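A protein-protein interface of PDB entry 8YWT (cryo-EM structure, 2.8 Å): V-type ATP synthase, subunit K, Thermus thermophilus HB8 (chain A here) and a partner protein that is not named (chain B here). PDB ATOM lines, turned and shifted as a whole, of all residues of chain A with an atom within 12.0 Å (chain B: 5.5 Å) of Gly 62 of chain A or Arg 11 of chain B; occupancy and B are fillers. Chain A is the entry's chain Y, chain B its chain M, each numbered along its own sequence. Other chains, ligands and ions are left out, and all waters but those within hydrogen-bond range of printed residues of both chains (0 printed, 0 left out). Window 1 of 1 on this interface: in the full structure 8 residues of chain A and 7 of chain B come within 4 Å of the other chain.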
ATOM      1  N   GLN A  53     -37.357  17.383 -27.958  1.00  0.00           N
ATOM      2  CA  GLN A  53     -36.237  18.153 -27.406  1.00  0.00           C
ATOM      3  C   GLN A  53     -36.180  18.186 -25.874  1.00  0.00           C
ATOM      4  O   GLN A  53     -35.092  18.363 -25.339  1.00  0.00           O
ATOM      5  CB  GLN A  53     -36.240  19.577 -27.971  1.00  0.00           C
ATOM      6  CG  GLN A  53     -35.804  19.600 -29.439  1.00  0.00           C
ATOM      7  CD  GLN A  53     -35.633  21.007 -29.999  1.00  0.00           C
ATOM      8  OE1 GLN A  53     -36.248  21.963 -29.573  1.00  0.00           O
ATOM      9  NE2 GLN A  53     -34.795  21.184 -30.988  1.00  0.00           N
ATOM     10  N   ALA A  54     -37.280  17.971 -25.152  1.00  0.00           N
ATOM     11  CA  ALA A  54     -37.303  18.019 -23.691  1.00  0.00           C
ATOM     12  C   ALA A  54     -36.356  17.007 -23.030  1.00  0.00           C
ATOM     13  O   ALA A  54     -35.443  17.400 -22.306  1.00  0.00           O
ATOM     14  CB  ALA A  54     -38.751  17.843 -23.236  1.00  0.00           C
ATOM     15  N   ARG A  55     -36.537  15.705 -23.282  1.00  0.00           N
ATOM     16  CA  ARG A  55     -35.682  14.636 -22.732  1.00  0.00           C
ATOM     17  C   ARG A  55     -34.284  14.629 -23.342  1.00  0.00           C
ATOM     18  O   ARG A  55     -33.303  14.437 -22.634  1.00  0.00           O
ATOM     19  CB  ARG A  55     -36.339  13.265 -22.926  1.00  0.00           C
ATOM     20  CG  ARG A  55     -37.494  12.960 -21.980  1.00  0.00           C
ATOM     21  CD  ARG A  55     -37.901  11.490 -22.115  1.00  0.00           C
ATOM     22  NE  ARG A  55     -38.744  11.063 -20.990  1.00  0.00           N
ATOM     23  CZ  ARG A  55     -40.047  11.179 -20.869  1.00  0.00           C
ATOM     24  NH1 ARG A  55     -40.624  10.855 -19.756  1.00  0.00           N
ATOM     25  NH2 ARG A  55     -40.803  11.622 -21.822  1.00  0.00           N
ATOM     26  N   ILE A  56     -34.165  14.885 -24.639  1.00  0.00           N
ATOM     27  CA  ILE A  56     -32.867  14.944 -25.324  1.00  0.00           C
ATOM     28  C   ILE A  56     -32.008  16.095 -24.784  1.00  0.00           C
ATOM     29  O   ILE A  56     -30.843  15.894 -24.468  1.00  0.00           O
ATOM     30  CB  ILE A  56     -33.051  15.015 -26.856  1.00  0.00           C
ATOM     31  CG1 ILE A  56     -33.797  13.770 -27.379  1.00  0.00           C
ATOM     32  CG2 ILE A  56     -31.681  15.120 -27.538  1.00  0.00           C
ATOM     33  CD1 ILE A  56     -34.167  13.816 -28.864  1.00  0.00           C
ATOM     34  N   GLY A  57     -32.559  17.289 -24.610  1.00  0.00           N
ATOM     35  CA  GLY A  57     -31.801  18.441 -24.133  1.00  0.00           C
ATOM     36  C   GLY A  57     -31.460  18.382 -22.650  1.00  0.00           C
ATOM     37  O   GLY A  57     -30.400  18.856 -22.278  1.00  0.00           O
ATOM     38  N   ALA A  58     -32.273  17.759 -21.797  1.00  0.00           N
ATOM     39  CA  ALA A  58     -31.895  17.496 -20.408  1.00  0.00           C
ATOM     40  C   ALA A  58     -30.731  16.492 -20.313  1.00  0.00           C
ATOM     41  O   ALA A  58     -29.763  16.714 -19.589  1.00  0.00           O
ATOM     42  CB  ALA A  58     -33.133  17.004 -19.668  1.00  0.00           C
ATOM     43  N   ALA A  59     -30.767  15.423 -21.107  1.00  0.00           N
ATOM     44  CA  ALA A  59     -29.671  14.471 -21.221  1.00  0.00           C
ATOM     45  C   ALA A  59     -28.407  15.084 -21.819  1.00  0.00           C
ATOM     46  O   ALA A  59     -27.318  14.806 -21.331  1.00  0.00           O
ATOM     47  CB  ALA A  59     -30.165  13.285 -22.038  1.00  0.00           C
ATOM     48  N   GLY A  60     -28.537  15.970 -22.807  1.00  0.00           N
ATOM     49  CA  GLY A  60     -27.444  16.739 -23.403  1.00  0.00           C
ATOM     50  C   GLY A  60     -26.792  17.710 -22.428  1.00  0.00           C
ATOM     51  O   GLY A  60     -25.587  17.629 -22.235  1.00  0.00           O
ATOM     52  N   VAL A  61     -27.552  18.567 -21.742  1.00  0.00           N
ATOM     53  CA  VAL A  61     -27.030  19.478 -20.703  1.00  0.00           C
ATOM     54  C   VAL A  61     -26.263  18.717 -19.624  1.00  0.00           C
ATOM     55  O   VAL A  61     -25.221  19.194 -19.180  1.00  0.00           O
ATOM     56  CB  VAL A  61     -28.165  20.318 -20.065  1.00  0.00           C
ATOM     57  CG1 VAL A  61     -27.749  21.088 -18.807  1.00  0.00           C
ATOM     58  CG2 VAL A  61     -28.697  21.375 -21.029  1.00  0.00           C
ATOM     59  N   GLY A  62     -26.740  17.532 -19.232  1.00  0.00           N
ATOM     60  CA  GLY A  62     -26.095  16.653 -18.254  1.00  0.00           C
ATOM     61  C   GLY A  62     -24.817  15.991 -18.749  1.00  0.00           C
ATOM     62  O   GLY A  62     -23.827  15.996 -18.031  1.00  0.00           O
ATOM     63  N   ALA A  63     -24.773  15.487 -19.978  1.00  0.00           N
ATOM     64  CA  ALA A  63     -23.528  14.991 -20.561  1.00  0.00           C
ATOM     65  C   ALA A  63     -22.465  16.097 -20.628  1.00  0.00           C
ATOM     66  O   ALA A  63     -21.359  15.905 -20.144  1.00  0.00           O
ATOM     67  CB  ALA A  63     -23.810  14.406 -21.943  1.00  0.00           C
ATOM     68  N   ILE A  64     -22.816  17.282 -21.131  1.00  0.00           N
ATOM     69  CA  ILE A  64     -21.908  18.433 -21.185  1.00  0.00           C
ATOM     70  C   ILE A  64     -21.467  18.872 -19.787  1.00  0.00           C
ATOM     71  O   ILE A  64     -20.321  19.252 -19.600  1.00  0.00           O
ATOM     72  CB  ILE A  64     -22.579  19.624 -21.897  1.00  0.00           C
ATOM     73  CG1 ILE A  64     -23.010  19.291 -23.331  1.00  0.00           C
ATOM     74  CG2 ILE A  64     -21.643  20.848 -21.942  1.00  0.00           C
ATOM     75  CD1 ILE A  64     -24.105  20.231 -23.839  1.00  0.00           C
ATOM     76  N   ALA A  65     -22.337  18.838 -18.775  1.00  0.00           N
ATOM     77  CA  ALA A  65     -21.959  19.219 -17.417  1.00  0.00           C
ATOM     78  C   ALA A  65     -20.866  18.308 -16.843  1.00  0.00           C
ATOM     79  O   ALA A  65     -19.936  18.791 -16.206  1.00  0.00           O
ATOM     80  CB  ALA A  65     -23.212  19.212 -16.542  1.00  0.00           C
ATOM     81  N   GLU A  66     -20.945  16.999 -17.081  1.00  0.00           N
ATOM     82  CA  GLU A  66     -19.954  16.042 -16.590  1.00  0.00           C
ATOM     83  C   GLU A  66     -18.651  16.036 -17.417  1.00  0.00           C
ATOM     84  O   GLU A  66     -17.578  15.783 -16.875  1.00  0.00           O
ATOM     85  CB  GLU A  66     -20.603  14.657 -16.517  1.00  0.00           C
ATOM     86  CG  GLU A  66     -19.880  13.684 -15.576  1.00  0.00           C
ATOM     87  CD  GLU A  66     -19.903  14.105 -14.100  1.00  0.00           C
ATOM     88  OE1 GLU A  66     -20.900  14.691 -13.628  1.00  0.00           O
ATOM     89  OE2 GLU A  66     -18.940  13.801 -13.368  1.00  0.00           O
ATOM     90  N   ASP A  67     -18.703  16.375 -18.706  1.00  0.00           N
ATOM     91  CA  ASP A  67     -17.531  16.583 -19.565  1.00  0.00           C
ATOM     92  C   ASP A  67     -17.836  17.587 -20.695  1.00  0.00           C
ATOM     93  O   ASP A  67     -18.597  17.301 -21.617  1.00  0.00           O
ATOM     94  CB  ASP A  67     -17.064  15.218 -20.086  1.00  0.00           C
ATOM     95  CG  ASP A  67     -15.858  15.269 -21.021  1.00  0.00           C
ATOM     96  OD1 ASP A  67     -15.475  16.353 -21.515  1.00  0.00           O
ATOM     97  OD2 ASP A  67     -15.278  14.199 -21.296  1.00  0.00           O
ATOM     98  N   ARG A  68     -17.203  18.771 -20.663  1.00  0.00           N
ATOM     99  CA  ARG A  68     -17.492  19.868 -21.606  1.00  0.00           C
ATOM    100  C   ARG A  68     -17.206  19.513 -23.066  1.00  0.00           C
ATOM    101  O   ARG A  68     -17.718  20.180 -23.953  1.00  0.00           O
ATOM    102  CB  ARG A  68     -16.775  21.166 -21.174  1.00  0.00           C
ATOM    103  CG  ARG A  68     -17.519  22.435 -21.652  1.00  0.00           C
ATOM    104  CD  ARG A  68     -16.830  23.772 -21.343  1.00  0.00           C
ATOM    105  NE  ARG A  68     -16.549  23.957 -19.908  1.00  0.00           N
ATOM    106  CZ  ARG A  68     -17.193  24.691 -19.018  1.00  0.00           C
ATOM    107  NH1 ARG A  68     -16.765  24.715 -17.793  1.00  0.00           N
ATOM    108  NH2 ARG A  68     -18.247  25.389 -19.317  1.00  0.00           N
ATOM    109  N   SER A  69     -16.458  18.448 -23.345  1.00  0.00           N
ATOM    110  CA  SER A  69     -16.235  17.955 -24.709  1.00  0.00           C
ATOM    111  C   SER A  69     -17.474  17.308 -25.350  1.00  0.00           C
ATOM    112  O   SER A  69     -17.519  17.178 -26.572  1.00  0.00           O
ATOM    113  CB  SER A  69     -15.080  16.957 -24.716  1.00  0.00           C
ATOM    114  OG  SER A  69     -15.467  15.771 -24.073  1.00  0.00           O
ATOM    115  N   ASN A  70     -18.503  16.924 -24.581  1.00  0.00           N
ATOM    116  CA  ASN A  70     -19.734  16.334 -25.123  1.00  0.00           C
ATOM    117  C   ASN A  70     -20.652  17.330 -25.865  1.00  0.00           C
ATOM    118  O   ASN A  70     -21.699  16.918 -26.358  1.00  0.00           O
ATOM    119  CB  ASN A  70     -20.478  15.566 -24.011  1.00  0.00           C
ATOM    120  CG  ASN A  70     -19.900  14.191 -23.733  1.00  0.00           C
ATOM    121  OD1 ASN A  70     -19.418  13.887 -22.660  1.00  0.00           O
ATOM    122  ND2 ASN A  70     -19.943  13.297 -24.691  1.00  0.00           N
ATOM    123  N   PHE A  71     -20.285  18.610 -25.982  1.00  0.00           N
ATOM    124  CA  PHE A  71     -21.103  19.674 -26.578  1.00  0.00           C
ATOM    125  C   PHE A  71     -21.571  19.394 -28.013  1.00  0.00           C
ATOM    126  O   PHE A  71     -22.763  19.489 -28.291  1.00  0.00           O
ATOM    127  CB  PHE A  71     -20.338  21.000 -26.464  1.00  0.00           C
ATOM    128  CG  PHE A  71     -21.150  22.222 -26.831  1.00  0.00           C
ATOM    129  CD1 PHE A  71     -22.022  22.794 -25.889  1.00  0.00           C
ATOM    130  CD2 PHE A  71     -21.042  22.796 -28.107  1.00  0.00           C
ATOM    131  CE1 PHE A  71     -22.794  23.915 -26.223  1.00  0.00           C
ATOM    132  CE2 PHE A  71     -21.812  23.921 -28.443  1.00  0.00           C
ATOM    133  CZ  PHE A  71     -22.696  24.475 -27.504  1.00  0.00           C
ATOM    134  N   GLY A  72     -20.682  18.980 -28.917  1.00  0.00           N
ATOM    135  CA  GLY A  72     -21.033  18.726 -30.319  1.00  0.00           C
ATOM    136  C   GLY A  72     -22.003  17.558 -30.522  1.00  0.00           C
ATOM    137  O   GLY A  72     -22.932  17.649 -31.319  1.00  0.00           O
ATOM    138  N   THR A  73     -21.863  16.479 -29.754  1.00  0.00           N
ATOM    139  CA  THR A  73     -22.788  15.330 -29.828  1.00  0.00           C
ATOM    140  C   THR A  73     -24.169  15.692 -29.292  1.00  0.00           C
ATOM    141  O   THR A  73     -25.181  15.353 -29.899  1.00  0.00           O
ATOM    142  CB  THR A  73     -22.225  14.122 -29.072  1.00  0.00           C
ATOM    143  OG1 THR A  73     -21.075  13.647 -29.728  1.00  0.00           O
ATOM    144  CG2 THR A  73     -23.200  12.948 -29.009  1.00  0.00           C
ATOM    145  N   ALA A  74     -24.219  16.426 -28.180  1.00  0.00           N
ATOM    146  CA  ALA A  74     -25.458  16.907 -27.589  1.00  0.00           C
ATOM    147  C   ALA A  74     -26.212  17.859 -28.527  1.00  0.00           C
ATOM    148  O   ALA A  74     -27.423  17.726 -28.669  1.00  0.00           O
ATOM    149  CB  ALA A  74     -25.100  17.556 -26.254  1.00  0.00           C
ATOM    150  N   LEU A  75     -25.519  18.766 -29.226  1.00  0.00           N
ATOM    151  CA  LEU A  75     -26.122  19.639 -30.236  1.00  0.00           C
ATOM    152  C   LEU A  75     -26.712  18.877 -31.423  1.00  0.00           C
ATOM    153  O   LEU A  75     -27.834  19.175 -31.814  1.00  0.00           O
ATOM    154  CB  LEU A  75     -25.085  20.642 -30.762  1.00  0.00           C
ATOM    155  CG  LEU A  75     -25.059  21.998 -30.055  1.00  0.00           C
ATOM    156  CD1 LEU A  75     -23.974  22.831 -30.717  1.00  0.00           C
ATOM    157  CD2 LEU A  75     -26.372  22.767 -30.207  1.00  0.00           C
ATOM    158  N   PHE A  77     -27.910  15.764 -31.629  1.00  0.00           N
ATOM    159  CA  PHE A  77     -29.136  15.097 -31.198  1.00  0.00           C
ATOM    160  C   PHE A  77     -30.252  16.087 -30.847  1.00  0.00           C
ATOM    161  O   PHE A  77     -31.405  15.788 -31.126  1.00  0.00           O
ATOM    162  CB  PHE A  77     -28.830  14.126 -30.050  1.00  0.00           C
ATOM    163  CG  PHE A  77     -28.322  12.767 -30.499  1.00  0.00           C
ATOM    164  CD1 PHE A  77     -27.126  12.647 -31.230  1.00  0.00           C
ATOM    165  CD2 PHE A  77     -29.069  11.609 -30.210  1.00  0.00           C
ATOM    166  CE1 PHE A  77     -26.718  11.400 -31.726  1.00  0.00           C
ATOM    167  CE2 PHE A  77     -28.656  10.357 -30.697  1.00  0.00           C
ATOM    168  CZ  PHE A  77     -27.492  10.258 -31.474  1.00  0.00           C
ATOM    169  N   LEU A  78     -29.958  17.275 -30.309  1.00  0.00           N
ATOM    170  CA  LEU A  78     -30.967  18.306 -30.036  1.00  0.00           C
ATOM    171  C   LEU A  78     -31.588  18.879 -31.319  1.00  0.00           C
ATOM    172  O   LEU A  78     -32.783  19.159 -31.360  1.00  0.00           O
ATOM    173  CB  LEU A  78     -30.320  19.418 -29.187  1.00  0.00           C
ATOM    174  CG  LEU A  78     -31.294  20.512 -28.717  1.00  0.00           C
ATOM    175  CD1 LEU A  78     -32.140  20.026 -27.548  1.00  0.00           C
ATOM    176  CD2 LEU A  78     -30.545  21.754 -28.265  1.00  0.00           C
ATOM    177  N   TYR B   7     -31.275  13.381 -17.380  1.00  0.00           N
ATOM    178  CA  TYR B   7     -30.126  14.190 -16.969  1.00  0.00           C
ATOM    179  C   TYR B   7     -29.134  13.402 -16.106  1.00  0.00           C
ATOM    180  O   TYR B   7     -27.967  13.313 -16.486  1.00  0.00           O
ATOM    181  CB  TYR B   7     -30.633  15.459 -16.271  1.00  0.00           C
ATOM    182  CG  TYR B   7     -29.627  16.193 -15.408  1.00  0.00           C
ATOM    183  CD1 TYR B   7     -28.678  17.054 -15.987  1.00  0.00           C
ATOM    184  CD2 TYR B   7     -29.672  16.046 -14.013  1.00  0.00           C
ATOM    185  CE1 TYR B   7     -27.772  17.765 -15.174  1.00  0.00           C
ATOM    186  CE2 TYR B   7     -28.770  16.749 -13.200  1.00  0.00           C
ATOM    187  CZ  TYR B   7     -27.819  17.612 -13.775  1.00  0.00           C
ATOM    188  OH  TYR B   7     -26.948  18.281 -12.977  1.00  0.00           O
ATOM    189  N   LEU B   8     -29.561  12.776 -14.996  1.00  0.00           N
ATOM    190  CA  LEU B   8     -28.626  12.082 -14.098  1.00  0.00           C
ATOM    191  C   LEU B   8     -27.922  10.922 -14.790  1.00  0.00           C
ATOM    192  O   LEU B   8     -26.715  10.765 -14.644  1.00  0.00           O
ATOM    193  CB  LEU B   8     -29.323  11.604 -12.812  1.00  0.00           C
ATOM    194  CG  LEU B   8     -28.392  10.827 -11.851  1.00  0.00           C
ATOM    195  CD1 LEU B   8     -27.256  11.678 -11.291  1.00  0.00           C
ATOM    196  CD2 LEU B   8     -29.158  10.265 -10.667  1.00  0.00           C
ATOM    197  N   ASN B   9     -28.631  10.125 -15.581  1.00  0.00           N
ATOM    198  CA  ASN B   9     -28.032   8.963 -16.216  1.00  0.00           C
ATOM    199  C   ASN B   9     -27.050   9.344 -17.320  1.00  0.00           C
ATOM    200  O   ASN B   9     -26.146   8.566 -17.580  1.00  0.00           O
ATOM    201  CB  ASN B   9     -29.104   7.970 -16.674  1.00  0.00           C
ATOM    202  CG  ASN B   9     -29.832   7.313 -15.515  1.00  0.00           C
ATOM    203  OD1 ASN B   9     -29.631   7.613 -14.357  1.00  0.00           O
ATOM    204  ND2 ASN B   9     -30.661   6.344 -15.784  1.00  0.00           N
ATOM    205  N   ALA B  10     -27.120  10.543 -17.903  1.00  0.00           N
ATOM    206  CA  ALA B  10     -26.074  11.035 -18.793  1.00  0.00           C
ATOM    207  C   ALA B  10     -24.766  11.321 -18.037  1.00  0.00           C
ATOM    208  O   ALA B  10     -23.696  10.962 -18.512  1.00  0.00           O
ATOM    209  CB  ALA B  10     -26.593  12.268 -19.516  1.00  0.00           C
ATOM    210  N   ARG B  11     -24.846  11.888 -16.827  1.00  0.00           N
ATOM    211  CA  ARG B  11     -23.705  12.091 -15.914  1.00  0.00           C
ATOM    212  C   ARG B  11     -23.134  10.774 -15.399  1.00  0.00           C
ATOM    213  O   ARG B  11     -21.925  10.585 -15.401  1.00  0.00           O
ATOM    214  CB  ARG B  11     -24.110  12.989 -14.735  1.00  0.00           C
ATOM    215  CG  ARG B  11     -24.652  14.344 -15.199  1.00  0.00           C
ATOM    216  CD  ARG B  11     -24.796  15.373 -14.079  1.00  0.00           C
ATOM    217  NE  ARG B  11     -23.479  15.795 -13.590  1.00  0.00           N
ATOM    218  CZ  ARG B  11     -23.088  16.972 -13.168  1.00  0.00           C
ATOM    219  NH1 ARG B  11     -21.851  17.130 -12.869  1.00  0.00           N
ATOM    220  NH2 ARG B  11     -23.848  18.011 -13.032  1.00  0.00           N
ATOM    221  N   VAL B  12     -23.983   9.818 -15.035  1.00  0.00           N
ATOM    222  CA  VAL B  12     -23.563   8.458 -14.664  1.00  0.00           C
ATOM    223  C   VAL B  12     -22.883   7.763 -15.837  1.00  0.00           C
ATOM    224  O   VAL B  12     -21.807   7.222 -15.646  1.00  0.00           O
ATOM    225  CB  VAL B  12     -24.738   7.642 -14.096  1.00  0.00           C
ATOM    226  CG1 VAL B  12     -24.437   6.156 -13.945  1.00  0.00           C
ATOM    227  CG2 VAL B  12     -25.146   8.169 -12.722  1.00  0.00           C
ATOM    228  N   ARG B  13     -23.412   7.828 -17.066  1.00  0.00           N
ATOM    229  CA  ARG B  13     -22.797   7.234 -18.274  1.00  0.00           C
ATOM    230  C   ARG B  13     -21.386   7.739 -18.533  1.00  0.00           C
ATOM    231  O   ARG B  13     -20.503   6.929 -18.784  1.00  0.00           O
ATOM    232  CB  ARG B  13     -23.662   7.518 -19.506  1.00  0.00           C
ATOM    233  CG  ARG B  13     -24.869   6.595 -19.650  1.00  0.00           C
ATOM    234  CD  ARG B  13     -24.475   5.211 -20.143  1.00  0.00           C
ATOM    235  NE  ARG B  13     -25.658   4.424 -20.498  1.00  0.00           N
ATOM    236  CZ  ARG B  13     -25.705   3.130 -20.707  1.00  0.00           C
ATOM    237  NH1 ARG B  13     -26.832   2.583 -21.025  1.00  0.00           N
ATOM    238  NH2 ARG B  13     -24.669   2.364 -20.594  1.00  0.00           N
ATOM    239  N   VAL B  14     -21.139   9.041 -18.411  1.00  0.00           N
ATOM    240  CA  VAL B  14     -19.786   9.610 -18.523  1.00  0.00           C
ATOM    241  C   VAL B  14     -18.827   8.971 -17.514  1.00  0.00           C
ATOM    242  O   VAL B  14     -17.725   8.575 -17.880  1.00  0.00           O
ATOM    243  CB  VAL B  14     -19.817  11.140 -18.357  1.00  0.00           C
ATOM    244  CG1 VAL B  14     -18.420  11.756 -18.286  1.00  0.00           C
ATOM    245  CG2 VAL B  14     -20.537  11.805 -19.524  1.00  0.00           C
ATOM    246  N   ARG B  15     -19.259   8.802 -16.258  1.00  0.00           N
ATOM    247  CA  ARG B  15     -18.476   8.172 -15.183  1.00  0.00           C
ATOM    248  C   ARG B  15     -18.279   6.668 -15.366  1.00  0.00           C
ATOM    249  O   ARG B  15     -17.193   6.178 -15.089  1.00  0.00           O
ATOM    250  CB  ARG B  15     -19.135   8.464 -13.833  1.00  0.00           C
ATOM    251  CG  ARG B  15     -19.092   9.950 -13.471  1.00  0.00           C
ATOM    252  CD  ARG B  15     -19.893  10.200 -12.195  1.00  0.00           C
ATOM    253  NE  ARG B  15     -19.854  11.618 -11.838  1.00  0.00           N
ATOM    254  CZ  ARG B  15     -20.189  12.183 -10.704  1.00  0.00           C
ATOM    255  NH1 ARG B  15     -20.156  13.469 -10.611  1.00  0.00           N
ATOM    256  NH2 ARG B  15     -20.541  11.500  -9.663  1.00  0.00           N
ATOM    257  N   ARG B  16     -19.261   5.928 -15.887  1.00  0.00           N
ATOM    258  CA  ARG B  16     -19.112   4.505 -16.271  1.00  0.00           C
ATOM    259  C   ARG B  16     -18.027   4.295 -17.324  1.00  0.00           C
ATOM    260  O   ARG B  16     -17.355   3.275 -17.313  1.00  0.00           O
ATOM    261  CB  ARG B  16     -20.434   3.911 -16.786  1.00  0.00           C
ATOM    262  CG  ARG B  16     -21.528   3.821 -15.719  1.00  0.00           C
ATOM    263  CD  ARG B  16     -22.683   2.898 -16.114  1.00  0.00           C
ATOM    264  NE  ARG B  16     -22.340   1.485 -15.882  1.00  0.00           N
ATOM    265  CZ  ARG B  16     -22.165   0.537 -16.771  1.00  0.00           C
ATOM    266  NH1 ARG B  16     -21.894  -0.656 -16.356  1.00  0.00           N
ATOM    267  NH2 ARG B  16     -22.233   0.732 -18.053  1.00  0.00           N
ATOM    268  N   LEU B  75     -26.486  16.205  -7.130  1.00  0.00           N
ATOM    269  CA  LEU B  75     -26.717  16.424  -8.563  1.00  0.00           C
ATOM    270  C   LEU B  75     -28.217  16.505  -8.887  1.00  0.00           C
ATOM    271  O   LEU B  75     -28.618  17.301  -9.730  1.00  0.00           O
ATOM    272  CB  LEU B  75     -26.047  15.280  -9.352  1.00  0.00           C
ATOM    273  CG  LEU B  75     -24.602  15.542  -9.814  1.00  0.00           C
ATOM    274  CD1 LEU B  75     -23.682  16.135  -8.759  1.00  0.00           C
ATOM    275  CD2 LEU B  75     -23.983  14.227 -10.278  1.00  0.00           C
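OH of Tyr 7 of chain B sits at hydrogen-bond distance from NH2 of Arg 11 of chain B, at 3.1 Å.
Gly 62 of chain A touches two residues of chain B.
Of chain A, only Ala 58 and Gly 62 come within 4 Å of Tyr 7 of chain B.
Val 12 of chain B touches none of the printed residues of chain A.
Val 14 of chain B touches two residues of chain A.
No residue of chain A comes within 4 Å of Leu 75 of chain B.
Printed residues of chain B within 4 Å of Glu 66 of chain A: Arg 11 (2.7 Å), Val 14 (3.6 Å) and Arg 15 (2.8 Å).
Of the printed residues of chain B, Ala 63 of chain A touches Ala 10.
Of the printed residues of chain B, Ala 58 of chain A touches Tyr 7.
Of the printed residues of chain B, Asn 70 of chain A touches Val 14.
Arg 16 of chain B touches none of the printed residues of chain A.
Thr 73 of chain A touches none of the printed residues of chain B.
The nearest residue of chain A that does not touch Arg 11 of chain B is Ala 63 of chain A (4.8 Å).
Tyr 7 of chain B touches Ala 58 of chain A.
Ala 59 of chain A touches Ala 10 of chain B (O to CB, 3.2 Å).
Tyr 7 of chain B touches Gly 62 of chain A (CD1 to CA, 3.5 Å).
Gly 62 of chain A touches Arg 11 of chain B (O to CG, 3.4 Å).
Ala 10 of chain B touches Ala 63 of chain A (CB to N, 3.7 Å).
Ala 65 of chain A touches Arg 11 of chain B.
Val 14 of chain B touches Glu 66 of chain A (CG1 to CG, 3.6 Å).
CG2 of Val 14 of chain B touches OD1 of Asn 70 of chain A, at 3.9 Å.
The guanidinium group (NH1) of Arg 11 of chain B lies within salt-bridge range of the side-chain carboxylate (OE1) of Glu 66 of chain A.
OE2 of Glu 66 of chain A is in salt-bridge range of NE of Arg 15 of chain B (2.8 Å).
Of the 11 printed residues of chain B, 5 touch a printed residue of chain A.
Hydrophobic or aromatic side chains of chain B that line the printed part of chain A: Tyr 7, Ala 10 and Val 14.
Of the 25 printed residues of chain A, 7 touch a printed residue of chain B.
Printed residues of chain A that touch a printed residue of chain B: Ala 58, Ala 59, Gly 62, Ala 63, Ala 65, Glu 66 and Asn 70.
Hydrophobic or aromatic side chains of chain A within 4 Å of the printed part of chain B: Ala 65.
Along chain A the printed residues that touch a printed residue of chain B span positions 58 to 70.
Among the printed residues, 10 pairs touch across the chains.
Among the printed residues, Asp or Glu carboxylates within 4 Å of a Lys or Arg side-chain nitrogen of the other chain: Glu 66 of chain A with Arg 11 of chain B (2.7 Å) and Glu 66 of chain A with Arg 15 of chain B (2.8 Å).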
